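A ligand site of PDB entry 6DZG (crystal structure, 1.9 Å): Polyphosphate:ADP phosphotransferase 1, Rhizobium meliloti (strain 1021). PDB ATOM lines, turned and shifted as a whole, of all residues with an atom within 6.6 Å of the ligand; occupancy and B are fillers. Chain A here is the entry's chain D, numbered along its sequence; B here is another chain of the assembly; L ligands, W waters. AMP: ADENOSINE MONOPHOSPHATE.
Merely in contact with the ligand: Arg 149, Phe 163, Met 222, Thr 119, Val 157 and Asp 223.
Hydrophobic or aromatic side chains within 4 Å of the ligand: Val 157, Phe 163 and Met 222.
Ten residues have an atom within 4 Å of the ligand: Thr 119, Lys 120, Arg 149, Asn 153, Val 157, Phe 163, Ser 220, Met 222, Asp 223 and Arg 111 of chain B.
Along chain A the residues within 4 Å of the ligand span positions 119 to 223.
NH2 of Arg 111 of chain B lies within salt-bridge range of OD1 of Asp 148, at 3.4 Å.
O of Asn 153 is in hydrogen-bond range of N of Glu 158 (3.1 Å).
The guanidinium group of Arg 149 is in salt-bridge range of the side-chain carboxylate of Asp 93, 2.7 Å away.
The backbone carbonyl oxygen (O) of Leu 118 sits at hydrogen-bond distance from the guanidinium group (NH1) of Arg 111 of chain B, at 2.9 Å.
The backbone carbonyl oxygen (O) of Thr 119 is in hydrogen-bond range of the guanidinium group (NH1) of Arg 133, at 2.7 Å.
The backbone NH (N) of Phe 163 sits at hydrogen-bond distance from the backbone carbonyl oxygen (O) of Glu 158 (2.9 Å).
The side-chain carboxylate (OD2) of Asp 223 lies within hydrogen-bond range of the backbone NH (N) of Ser 220, 3.0 Å away.
N of Arg 111 of chain B is in hydrogen-bond range of OD1 of Asn 109 of chain B, at 2.9 Å.
The guanidinium group (NE) of Arg 111 of chain B lies within salt-bridge range of an oxygen (O2P) of the ligand (3.4 Å).
The side-chain amide nitrogen (ND2) of Asn 153 is in hydrogen-bond range of an oxygen (O3') of the ligand (3.0 Å).
The backbone NH of Lys 120 is in hydrogen-bond range of an oxygen (O2') of the ligand (3.5 Å).
OG of Ser 220 lies within hydrogen-bond range of O3P of the ligand (2.6 Å).
Water W3 lies within hydrogen-bond range of an oxygen (O2P) of the ligand (2.8 Å), the guanidinium group of Arg 149 (2.9 Å) and the guanidinium group of Arg 111 of chain B (3.0 Å).
Water W6 lies within hydrogen-bond range of the backbone carbonyl oxygen of Leu 118, an oxygen (O3') of the ligand and the side-chain amide nitrogen of Asn 153.
Water W5 bridges an oxygen (O2') of the ligand (2.8 Å) and the backbone NH (N) of Lys 120 (3.4 Å).
Water W1 lies within hydrogen-bond range of OE2 of Glu 158, ND2 of Asn 153 and N3 of the ligand.
Water W4 lies within hydrogen-bond range of an oxygen (O2') of the ligand, the guanidinium group (NH2) of Arg 133, the backbone carbonyl oxygen (O) of Thr 119 and the side-chain amide nitrogen (ND2) of Asn 153.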
ATOM      1  N   ASP A  93      12.516 -30.146   6.807  1.00  0.00           N
ATOM      2  CA  ASP A  93      12.307 -30.858   5.561  1.00  0.00           C
ATOM      3  C   ASP A  93      11.706 -32.226   5.890  1.00  0.00           C
ATOM      4  O   ASP A  93      12.062 -32.848   6.886  1.00  0.00           O
ATOM      5  CB  ASP A  93      13.613 -30.979   4.789  1.00  0.00           C
ATOM      6  CG  ASP A  93      14.109 -29.621   4.278  1.00  0.00           C
ATOM      7  OD1 ASP A  93      13.296 -28.857   3.709  1.00  0.00           O
ATOM      8  OD2 ASP A  93      15.294 -29.293   4.469  1.00  0.00           O
ATOM      9  N   LEU A 118       6.376 -21.070  -4.923  1.00  0.00           N
ATOM     10  CA  LEU A 118       7.253 -20.355  -5.856  1.00  0.00           C
ATOM     11  C   LEU A 118       8.530 -21.156  -6.089  1.00  0.00           C
ATOM     12  O   LEU A 118       8.946 -21.956  -5.246  1.00  0.00           O
ATOM     13  CB  LEU A 118       7.606 -18.957  -5.325  1.00  0.00           C
ATOM     14  CG  LEU A 118       6.485 -17.939  -5.050  1.00  0.00           C
ATOM     15  CD1 LEU A 118       7.043 -16.553  -4.825  1.00  0.00           C
ATOM     16  CD2 LEU A 118       5.517 -17.933  -6.186  1.00  0.00           C
ATOM     17  N   THR A 119       9.150 -20.923  -7.238  1.00  0.00           N
ATOM     18  CA  THR A 119      10.440 -21.519  -7.560  1.00  0.00           C
ATOM     19  C   THR A 119      11.539 -20.507  -7.237  1.00  0.00           C
ATOM     20  O   THR A 119      11.281 -19.414  -6.735  1.00  0.00           O
ATOM     21  CB  THR A 119      10.479 -21.939  -9.038  1.00  0.00           C
ATOM     22  OG1 THR A 119      10.213 -20.801  -9.862  1.00  0.00           O
ATOM     23  CG2 THR A 119       9.442 -23.057  -9.313  1.00  0.00           C
ATOM     24  N   LYS A 120      12.795 -20.891  -7.512  1.00  0.00           N
ATOM     25  CA  LYS A 120      13.895 -20.008  -7.163  1.00  0.00           C
ATOM     26  C   LYS A 120      13.772 -18.693  -7.939  1.00  0.00           C
ATOM     27  O   LYS A 120      13.272 -18.672  -9.064  1.00  0.00           O
ATOM     28  CB  LYS A 120      15.245 -20.673  -7.418  1.00  0.00           C
ATOM     29  CG  LYS A 120      15.566 -20.979  -8.873  1.00  0.00           C
ATOM     30  CD  LYS A 120      16.939 -21.621  -8.999  1.00  0.00           C
ATOM     31  CE  LYS A 120      17.461 -21.505 -10.433  1.00  0.00           C
ATOM     32  NZ  LYS A 120      18.914 -21.845 -10.545  1.00  0.00           N
ATOM     33  N   PRO A 121      14.203 -17.585  -7.348  1.00  0.00           N
ATOM     34  CA  PRO A 121      13.991 -16.275  -7.987  1.00  0.00           C
ATOM     35  C   PRO A 121      14.779 -16.103  -9.276  1.00  0.00           C
ATOM     36  O   PRO A 121      15.924 -16.562  -9.404  1.00  0.00           O
ATOM     37  CB  PRO A 121      14.434 -15.271  -6.915  1.00  0.00           C
ATOM     38  CG  PRO A 121      15.360 -16.063  -6.022  1.00  0.00           C
ATOM     39  CD  PRO A 121      14.771 -17.446  -5.993  1.00  0.00           C
ATOM     40  N   ARG A 133       7.793 -10.317  -4.858  1.00  0.00           N
ATOM     41  CA  ARG A 133       7.181 -11.437  -5.550  1.00  0.00           C
ATOM     42  C   ARG A 133       6.184 -12.198  -4.685  1.00  0.00           C
ATOM     43  O   ARG A 133       5.362 -12.927  -5.221  1.00  0.00           O
ATOM     44  CB  ARG A 133       8.257 -12.390  -6.067  1.00  0.00           C
ATOM     45  CG  ARG A 133       8.978 -13.234  -4.996  1.00  0.00           C
ATOM     46  CD  ARG A 133       9.954 -14.151  -5.724  1.00  0.00           C
ATOM     47  NE  ARG A 133      10.579 -15.164  -4.886  1.00  0.00           N
ATOM     48  CZ  ARG A 133      10.907 -16.387  -5.299  1.00  0.00           C
ATOM     49  NH1 ARG A 133      10.636 -16.761  -6.539  1.00  0.00           N
ATOM     50  NH2 ARG A 133      11.497 -17.229  -4.474  1.00  0.00           N
ATOM     51  N   TYR A 134       6.245 -12.044  -3.356  1.00  0.00           N
ATOM     52  CA  TYR A 134       5.209 -12.622  -2.508  1.00  0.00           C
ATOM     53  C   TYR A 134       3.971 -11.748  -2.440  1.00  0.00           C
ATOM     54  O   TYR A 134       2.843 -12.253  -2.370  1.00  0.00           O
ATOM     55  CB  TYR A 134       5.753 -12.879  -1.100  1.00  0.00           C
ATOM     56  CG  TYR A 134       6.790 -13.980  -1.132  1.00  0.00           C
ATOM     57  CD1 TYR A 134       6.397 -15.317  -1.147  1.00  0.00           C
ATOM     58  CD2 TYR A 134       8.141 -13.686  -1.210  1.00  0.00           C
ATOM     59  CE1 TYR A 134       7.337 -16.349  -1.219  1.00  0.00           C
ATOM     60  CE2 TYR A 134       9.104 -14.718  -1.276  1.00  0.00           C
ATOM     61  CZ  TYR A 134       8.689 -16.032  -1.273  1.00  0.00           C
ATOM     62  OH  TYR A 134       9.627 -17.030  -1.357  1.00  0.00           O
ATOM     63  N   ASP A 148       3.196 -22.854   0.448  1.00  0.00           N
ATOM     64  CA  ASP A 148       4.046 -24.038   0.580  1.00  0.00           C
ATOM     65  C   ASP A 148       5.494 -23.547   0.530  1.00  0.00           C
ATOM     66  O   ASP A 148       6.115 -23.480  -0.537  1.00  0.00           O
ATOM     67  CB  ASP A 148       3.712 -25.037  -0.525  1.00  0.00           C
ATOM     68  CG  ASP A 148       4.585 -26.285  -0.493  1.00  0.00           C
ATOM     69  OD1 ASP A 148       5.452 -26.413   0.394  1.00  0.00           O
ATOM     70  OD2 ASP A 148       4.400 -27.146  -1.385  1.00  0.00           O
ATOM     71  N   ARG A 149       6.028 -23.189   1.713  1.00  0.00           N
ATOM     72  CA  ARG A 149       7.187 -22.314   1.913  1.00  0.00           C
ATOM     73  C   ARG A 149       6.801 -20.888   1.569  1.00  0.00           C
ATOM     74  O   ARG A 149       5.774 -20.664   0.905  1.00  0.00           O
ATOM     75  CB  ARG A 149       8.388 -22.723   1.073  1.00  0.00           C
ATOM     76  CG  ARG A 149       8.956 -24.065   1.404  1.00  0.00           C
ATOM     77  CD  ARG A 149      10.239 -24.282   0.618  1.00  0.00           C
ATOM     78  NE  ARG A 149      10.755 -25.617   0.870  1.00  0.00           N
ATOM     79  CZ  ARG A 149      11.686 -25.907   1.772  1.00  0.00           C
ATOM     80  NH1 ARG A 149      12.201 -24.938   2.528  1.00  0.00           N
ATOM     81  NH2 ARG A 149      12.092 -27.161   1.918  1.00  0.00           N
ATOM     82  N   ASN A 153      11.825 -18.547   3.437  1.00  0.00           N
ATOM     83  CA  ASN A 153      13.018 -19.109   2.773  1.00  0.00           C
ATOM     84  C   ASN A 153      14.289 -18.400   3.251  1.00  0.00           C
ATOM     85  O   ASN A 153      15.317 -19.044   3.507  1.00  0.00           O
ATOM     86  CB  ASN A 153      12.886 -18.992   1.250  1.00  0.00           C
ATOM     87  CG  ASN A 153      12.149 -20.158   0.642  1.00  0.00           C
ATOM     88  OD1 ASN A 153      11.274 -20.754   1.270  1.00  0.00           O
ATOM     89  ND2 ASN A 153      12.515 -20.510  -0.588  1.00  0.00           N
ATOM     90  N   VAL A 157      16.376 -22.128   4.354  1.00  0.00           N
ATOM     91  CA  VAL A 157      17.135 -22.768   3.283  1.00  0.00           C
ATOM     92  C   VAL A 157      18.170 -21.818   2.667  1.00  0.00           C
ATOM     93  O   VAL A 157      19.305 -22.226   2.370  1.00  0.00           O
ATOM     94  CB  VAL A 157      16.180 -23.344   2.208  1.00  0.00           C
ATOM     95  CG1 VAL A 157      15.394 -22.259   1.515  1.00  0.00           C
ATOM     96  CG2 VAL A 157      16.978 -24.203   1.211  1.00  0.00           C
ATOM     97  N   GLU A 158      17.824 -20.546   2.481  1.00  0.00           N
ATOM     98  CA  GLU A 158      18.779 -19.630   1.849  1.00  0.00           C
ATOM     99  C   GLU A 158      20.048 -19.416   2.673  1.00  0.00           C
ATOM    100  O   GLU A 158      21.147 -19.630   2.149  1.00  0.00           O
ATOM    101  CB  GLU A 158      18.126 -18.292   1.503  1.00  0.00           C
ATOM    102  CG  GLU A 158      16.949 -18.368   0.503  1.00  0.00           C
ATOM    103  CD  GLU A 158      16.553 -17.005  -0.033  1.00  0.00           C
ATOM    104  OE1 GLU A 158      17.097 -16.004   0.489  1.00  0.00           O
ATOM    105  OE2 GLU A 158      15.720 -16.921  -0.964  1.00  0.00           O
ATOM    106  N   PHE A 163      22.437 -19.250  -0.387  1.00  0.00           N
ATOM    107  CA  PHE A 163      21.735 -18.545  -1.454  1.00  0.00           C
ATOM    108  C   PHE A 163      21.452 -17.102  -1.109  1.00  0.00           C
ATOM    109  O   PHE A 163      20.883 -16.378  -1.938  1.00  0.00           O
ATOM    110  CB  PHE A 163      20.409 -19.222  -1.781  1.00  0.00           C
ATOM    111  CG  PHE A 163      20.514 -20.666  -2.125  1.00  0.00           C
ATOM    112  CD1 PHE A 163      21.524 -21.133  -2.939  1.00  0.00           C
ATOM    113  CD2 PHE A 163      19.580 -21.573  -1.630  1.00  0.00           C
ATOM    114  CE1 PHE A 163      21.600 -22.471  -3.261  1.00  0.00           C
ATOM    115  CE2 PHE A 163      19.658 -22.908  -1.943  1.00  0.00           C
ATOM    116  CZ  PHE A 163      20.675 -23.364  -2.752  1.00  0.00           C
ATOM    117  N   LYS A 218       9.200 -36.386  -3.887  1.00  0.00           N
ATOM    118  CA  LYS A 218       9.284 -35.521  -2.727  1.00  0.00           C
ATOM    119  C   LYS A 218      10.714 -35.239  -2.285  1.00  0.00           C
ATOM    120  O   LYS A 218      10.926 -34.375  -1.432  1.00  0.00           O
ATOM    121  CB  LYS A 218       8.494 -36.139  -1.565  1.00  0.00           C
ATOM    122  CG  LYS A 218       6.970 -36.081  -1.725  1.00  0.00           C
ATOM    123  CD  LYS A 218       6.268 -36.669  -0.516  1.00  0.00           C
ATOM    124  CE  LYS A 218       4.763 -36.772  -0.717  1.00  0.00           C
ATOM    125  NZ  LYS A 218       4.073 -37.360   0.479  1.00  0.00           N
ATOM    126  N   LEU A 219      11.696 -35.947  -2.842  1.00  0.00           N
ATOM    127  CA  LEU A 219      13.091 -35.691  -2.525  1.00  0.00           C
ATOM    128  C   LEU A 219      13.686 -34.713  -3.522  1.00  0.00           C
ATOM    129  O   LEU A 219      13.277 -34.660  -4.675  1.00  0.00           O
ATOM    130  CB  LEU A 219      13.920 -36.975  -2.547  1.00  0.00           C
ATOM    131  CG  LEU A 219      13.929 -37.897  -1.330  1.00  0.00           C
ATOM    132  CD1 LEU A 219      15.057 -38.917  -1.497  1.00  0.00           C
ATOM    133  CD2 LEU A 219      14.143 -37.100  -0.063  1.00  0.00           C
ATOM    134  N   SER A 220      14.666 -33.943  -3.064  1.00  0.00           N
ATOM    135  CA  SER A 220      15.309 -32.934  -3.886  1.00  0.00           C
ATOM    136  C   SER A 220      16.761 -32.828  -3.459  1.00  0.00           C
ATOM    137  O   SER A 220      17.106 -33.232  -2.348  1.00  0.00           O
ATOM    138  CB  SER A 220      14.618 -31.572  -3.736  1.00  0.00           C
ATOM    139  OG  SER A 220      15.029 -30.955  -2.526  1.00  0.00           O
ATOM    140  N   PRO A 221      17.623 -32.304  -4.329  1.00  0.00           N
ATOM    141  CA  PRO A 221      19.001 -32.011  -3.881  1.00  0.00           C
ATOM    142  C   PRO A 221      19.046 -31.183  -2.614  1.00  0.00           C
ATOM    143  O   PRO A 221      19.964 -31.347  -1.810  1.00  0.00           O
ATOM    144  CB  PRO A 221      19.592 -31.260  -5.086  1.00  0.00           C
ATOM    145  CG  PRO A 221      18.817 -31.760  -6.268  1.00  0.00           C
ATOM    146  CD  PRO A 221      17.419 -31.992  -5.759  1.00  0.00           C
ATOM    147  N   MET A 222      18.067 -30.301  -2.403  1.00  0.00           N
ATOM    148  CA  MET A 222      17.946 -29.533  -1.157  1.00  0.00           C
ATOM    149  C   MET A 222      17.752 -30.440   0.061  1.00  0.00           C
ATOM    150  O   MET A 222      18.350 -30.215   1.108  1.00  0.00           O
ATOM    151  CB  MET A 222      16.770 -28.548  -1.228  1.00  0.00           C
ATOM    152  CG  MET A 222      16.986 -27.401  -2.192  1.00  0.00           C
ATOM    153  SD  MET A 222      18.656 -26.471  -1.819  1.00  0.00           S
ATOM    154  CE  MET A 222      19.794 -27.257  -3.191  1.00  0.00           C
ATOM    155  N   ASP A 223      16.888 -31.443  -0.095  1.00  0.00           N
ATOM    156  CA  ASP A 223      16.688 -32.427   0.958  1.00  0.00           C
ATOM    157  C   ASP A 223      17.975 -33.222   1.219  1.00  0.00           C
ATOM    158  O   ASP A 223      18.327 -33.462   2.387  1.00  0.00           O
ATOM    159  CB  ASP A 223      15.550 -33.371   0.595  1.00  0.00           C
ATOM    160  CG  ASP A 223      14.209 -32.655   0.493  1.00  0.00           C
ATOM    161  OD1 ASP A 223      13.808 -31.993   1.474  1.00  0.00           O
ATOM    162  OD2 ASP A 223      13.576 -32.730  -0.581  1.00  0.00           O
ATOM    163  N   ASN B 109       4.886 -32.687  -8.112  1.00  0.00           N
ATOM    164  CA  ASN B 109       5.522 -31.583  -7.397  1.00  0.00           C
ATOM    165  C   ASN B 109       4.734 -30.284  -7.605  1.00  0.00           C
ATOM    166  O   ASN B 109       4.577 -29.862  -8.749  1.00  0.00           O
ATOM    167  CB  ASN B 109       6.956 -31.426  -7.906  1.00  0.00           C
ATOM    168  CG  ASN B 109       7.816 -30.521  -7.042  1.00  0.00           C
ATOM    169  OD1 ASN B 109       7.344 -29.507  -6.534  1.00  0.00           O
ATOM    170  ND2 ASN B 109       9.086 -30.896  -6.890  1.00  0.00           N
ATOM    171  N   ARG B 111       5.644 -27.322  -7.348  1.00  0.00           N
ATOM    172  CA  ARG B 111       6.411 -26.253  -7.967  1.00  0.00           C
ATOM    173  C   ARG B 111       6.597 -26.419  -9.470  1.00  0.00           C
ATOM    174  O   ARG B 111       7.143 -25.518 -10.114  1.00  0.00           O
ATOM    175  CB  ARG B 111       7.789 -26.138  -7.280  1.00  0.00           C
ATOM    176  CG  ARG B 111       7.658 -25.697  -5.825  1.00  0.00           C
ATOM    177  CD  ARG B 111       8.988 -25.466  -5.095  1.00  0.00           C
ATOM    178  NE  ARG B 111       8.771 -25.774  -3.682  1.00  0.00           N
ATOM    179  CZ  ARG B 111       8.166 -24.954  -2.828  1.00  0.00           C
ATOM    180  NH1 ARG B 111       7.753 -23.745  -3.227  1.00  0.00           N
ATOM    181  NH2 ARG B 111       7.969 -25.352  -1.570  1.00  0.00           N
HETATM  182  P   AMP L   1      12.771 -28.080  -3.107  1.00  0.00           P
HETATM  183  O1P AMP L   1      13.171 -28.482  -4.499  1.00  0.00           O
HETATM  184  O2P AMP L   1      11.302 -27.867  -2.804  1.00  0.00           O
HETATM  185  O3P AMP L   1      13.261 -29.092  -2.102  1.00  0.00           O
HETATM  186  O5' AMP L   1      13.568 -26.723  -2.842  1.00  0.00           O
HETATM  187  C5' AMP L   1      13.696 -26.194  -1.524  1.00  0.00           C
HETATM  188  C4' AMP L   1      13.494 -24.698  -1.539  1.00  0.00           C
HETATM  189  O4' AMP L   1      14.769 -24.067  -1.867  1.00  0.00           O
HETATM  190  C3' AMP L   1      12.492 -24.210  -2.576  1.00  0.00           C
HETATM  191  O3' AMP L   1      11.794 -23.067  -2.072  1.00  0.00           O
HETATM  192  C2' AMP L   1      13.395 -23.788  -3.730  1.00  0.00           C
HETATM  193  O2' AMP L   1      12.835 -22.823  -4.606  1.00  0.00           O
HETATM  194  C1' AMP L   1      14.599 -23.228  -2.989  1.00  0.00           C
HETATM  195  N9  AMP L   1      15.824 -23.217  -3.805  1.00  0.00           N
HETATM  196  C8  AMP L   1      16.331 -24.242  -4.500  1.00  0.00           C
HETATM  197  N7  AMP L   1      17.421 -23.813  -5.162  1.00  0.00           N
HETATM  198  C5  AMP L   1      17.593 -22.514  -4.885  1.00  0.00           C
HETATM  199  C6  AMP L   1      18.536 -21.587  -5.301  1.00  0.00           C
HETATM  200  N6  AMP L   1      19.614 -21.969  -6.193  1.00  0.00           N
HETATM  201  N1  AMP L   1      18.458 -20.341  -4.880  1.00  0.00           N
HETATM  202  C2  AMP L   1      17.463 -19.963  -4.047  1.00  0.00           C
HETATM  203  N3  AMP L   1      16.545 -20.868  -3.632  1.00  0.00           N
HETATM  204  C4  AMP L   1      16.594 -22.143  -4.070  1.00  0.00           C
HETATM  205  O   HOH W   1      14.728 -19.294  -1.878  1.00  0.00           O
HETATM  206  O   HOH W   2      19.079 -17.474  -5.767  1.00  0.00           O
HETATM  207  O   HOH W   3       9.509 -27.771  -0.682  1.00  0.00           O
HETATM  208  O   HOH W   4      12.791 -19.893  -3.904  1.00  0.00           O
HETATM  209  O   HOH W   5      12.362 -24.216  -7.002  1.00  0.00           O
HETATM  210  O   HOH W   6      10.324 -20.901  -3.096  1.00  0.00           O
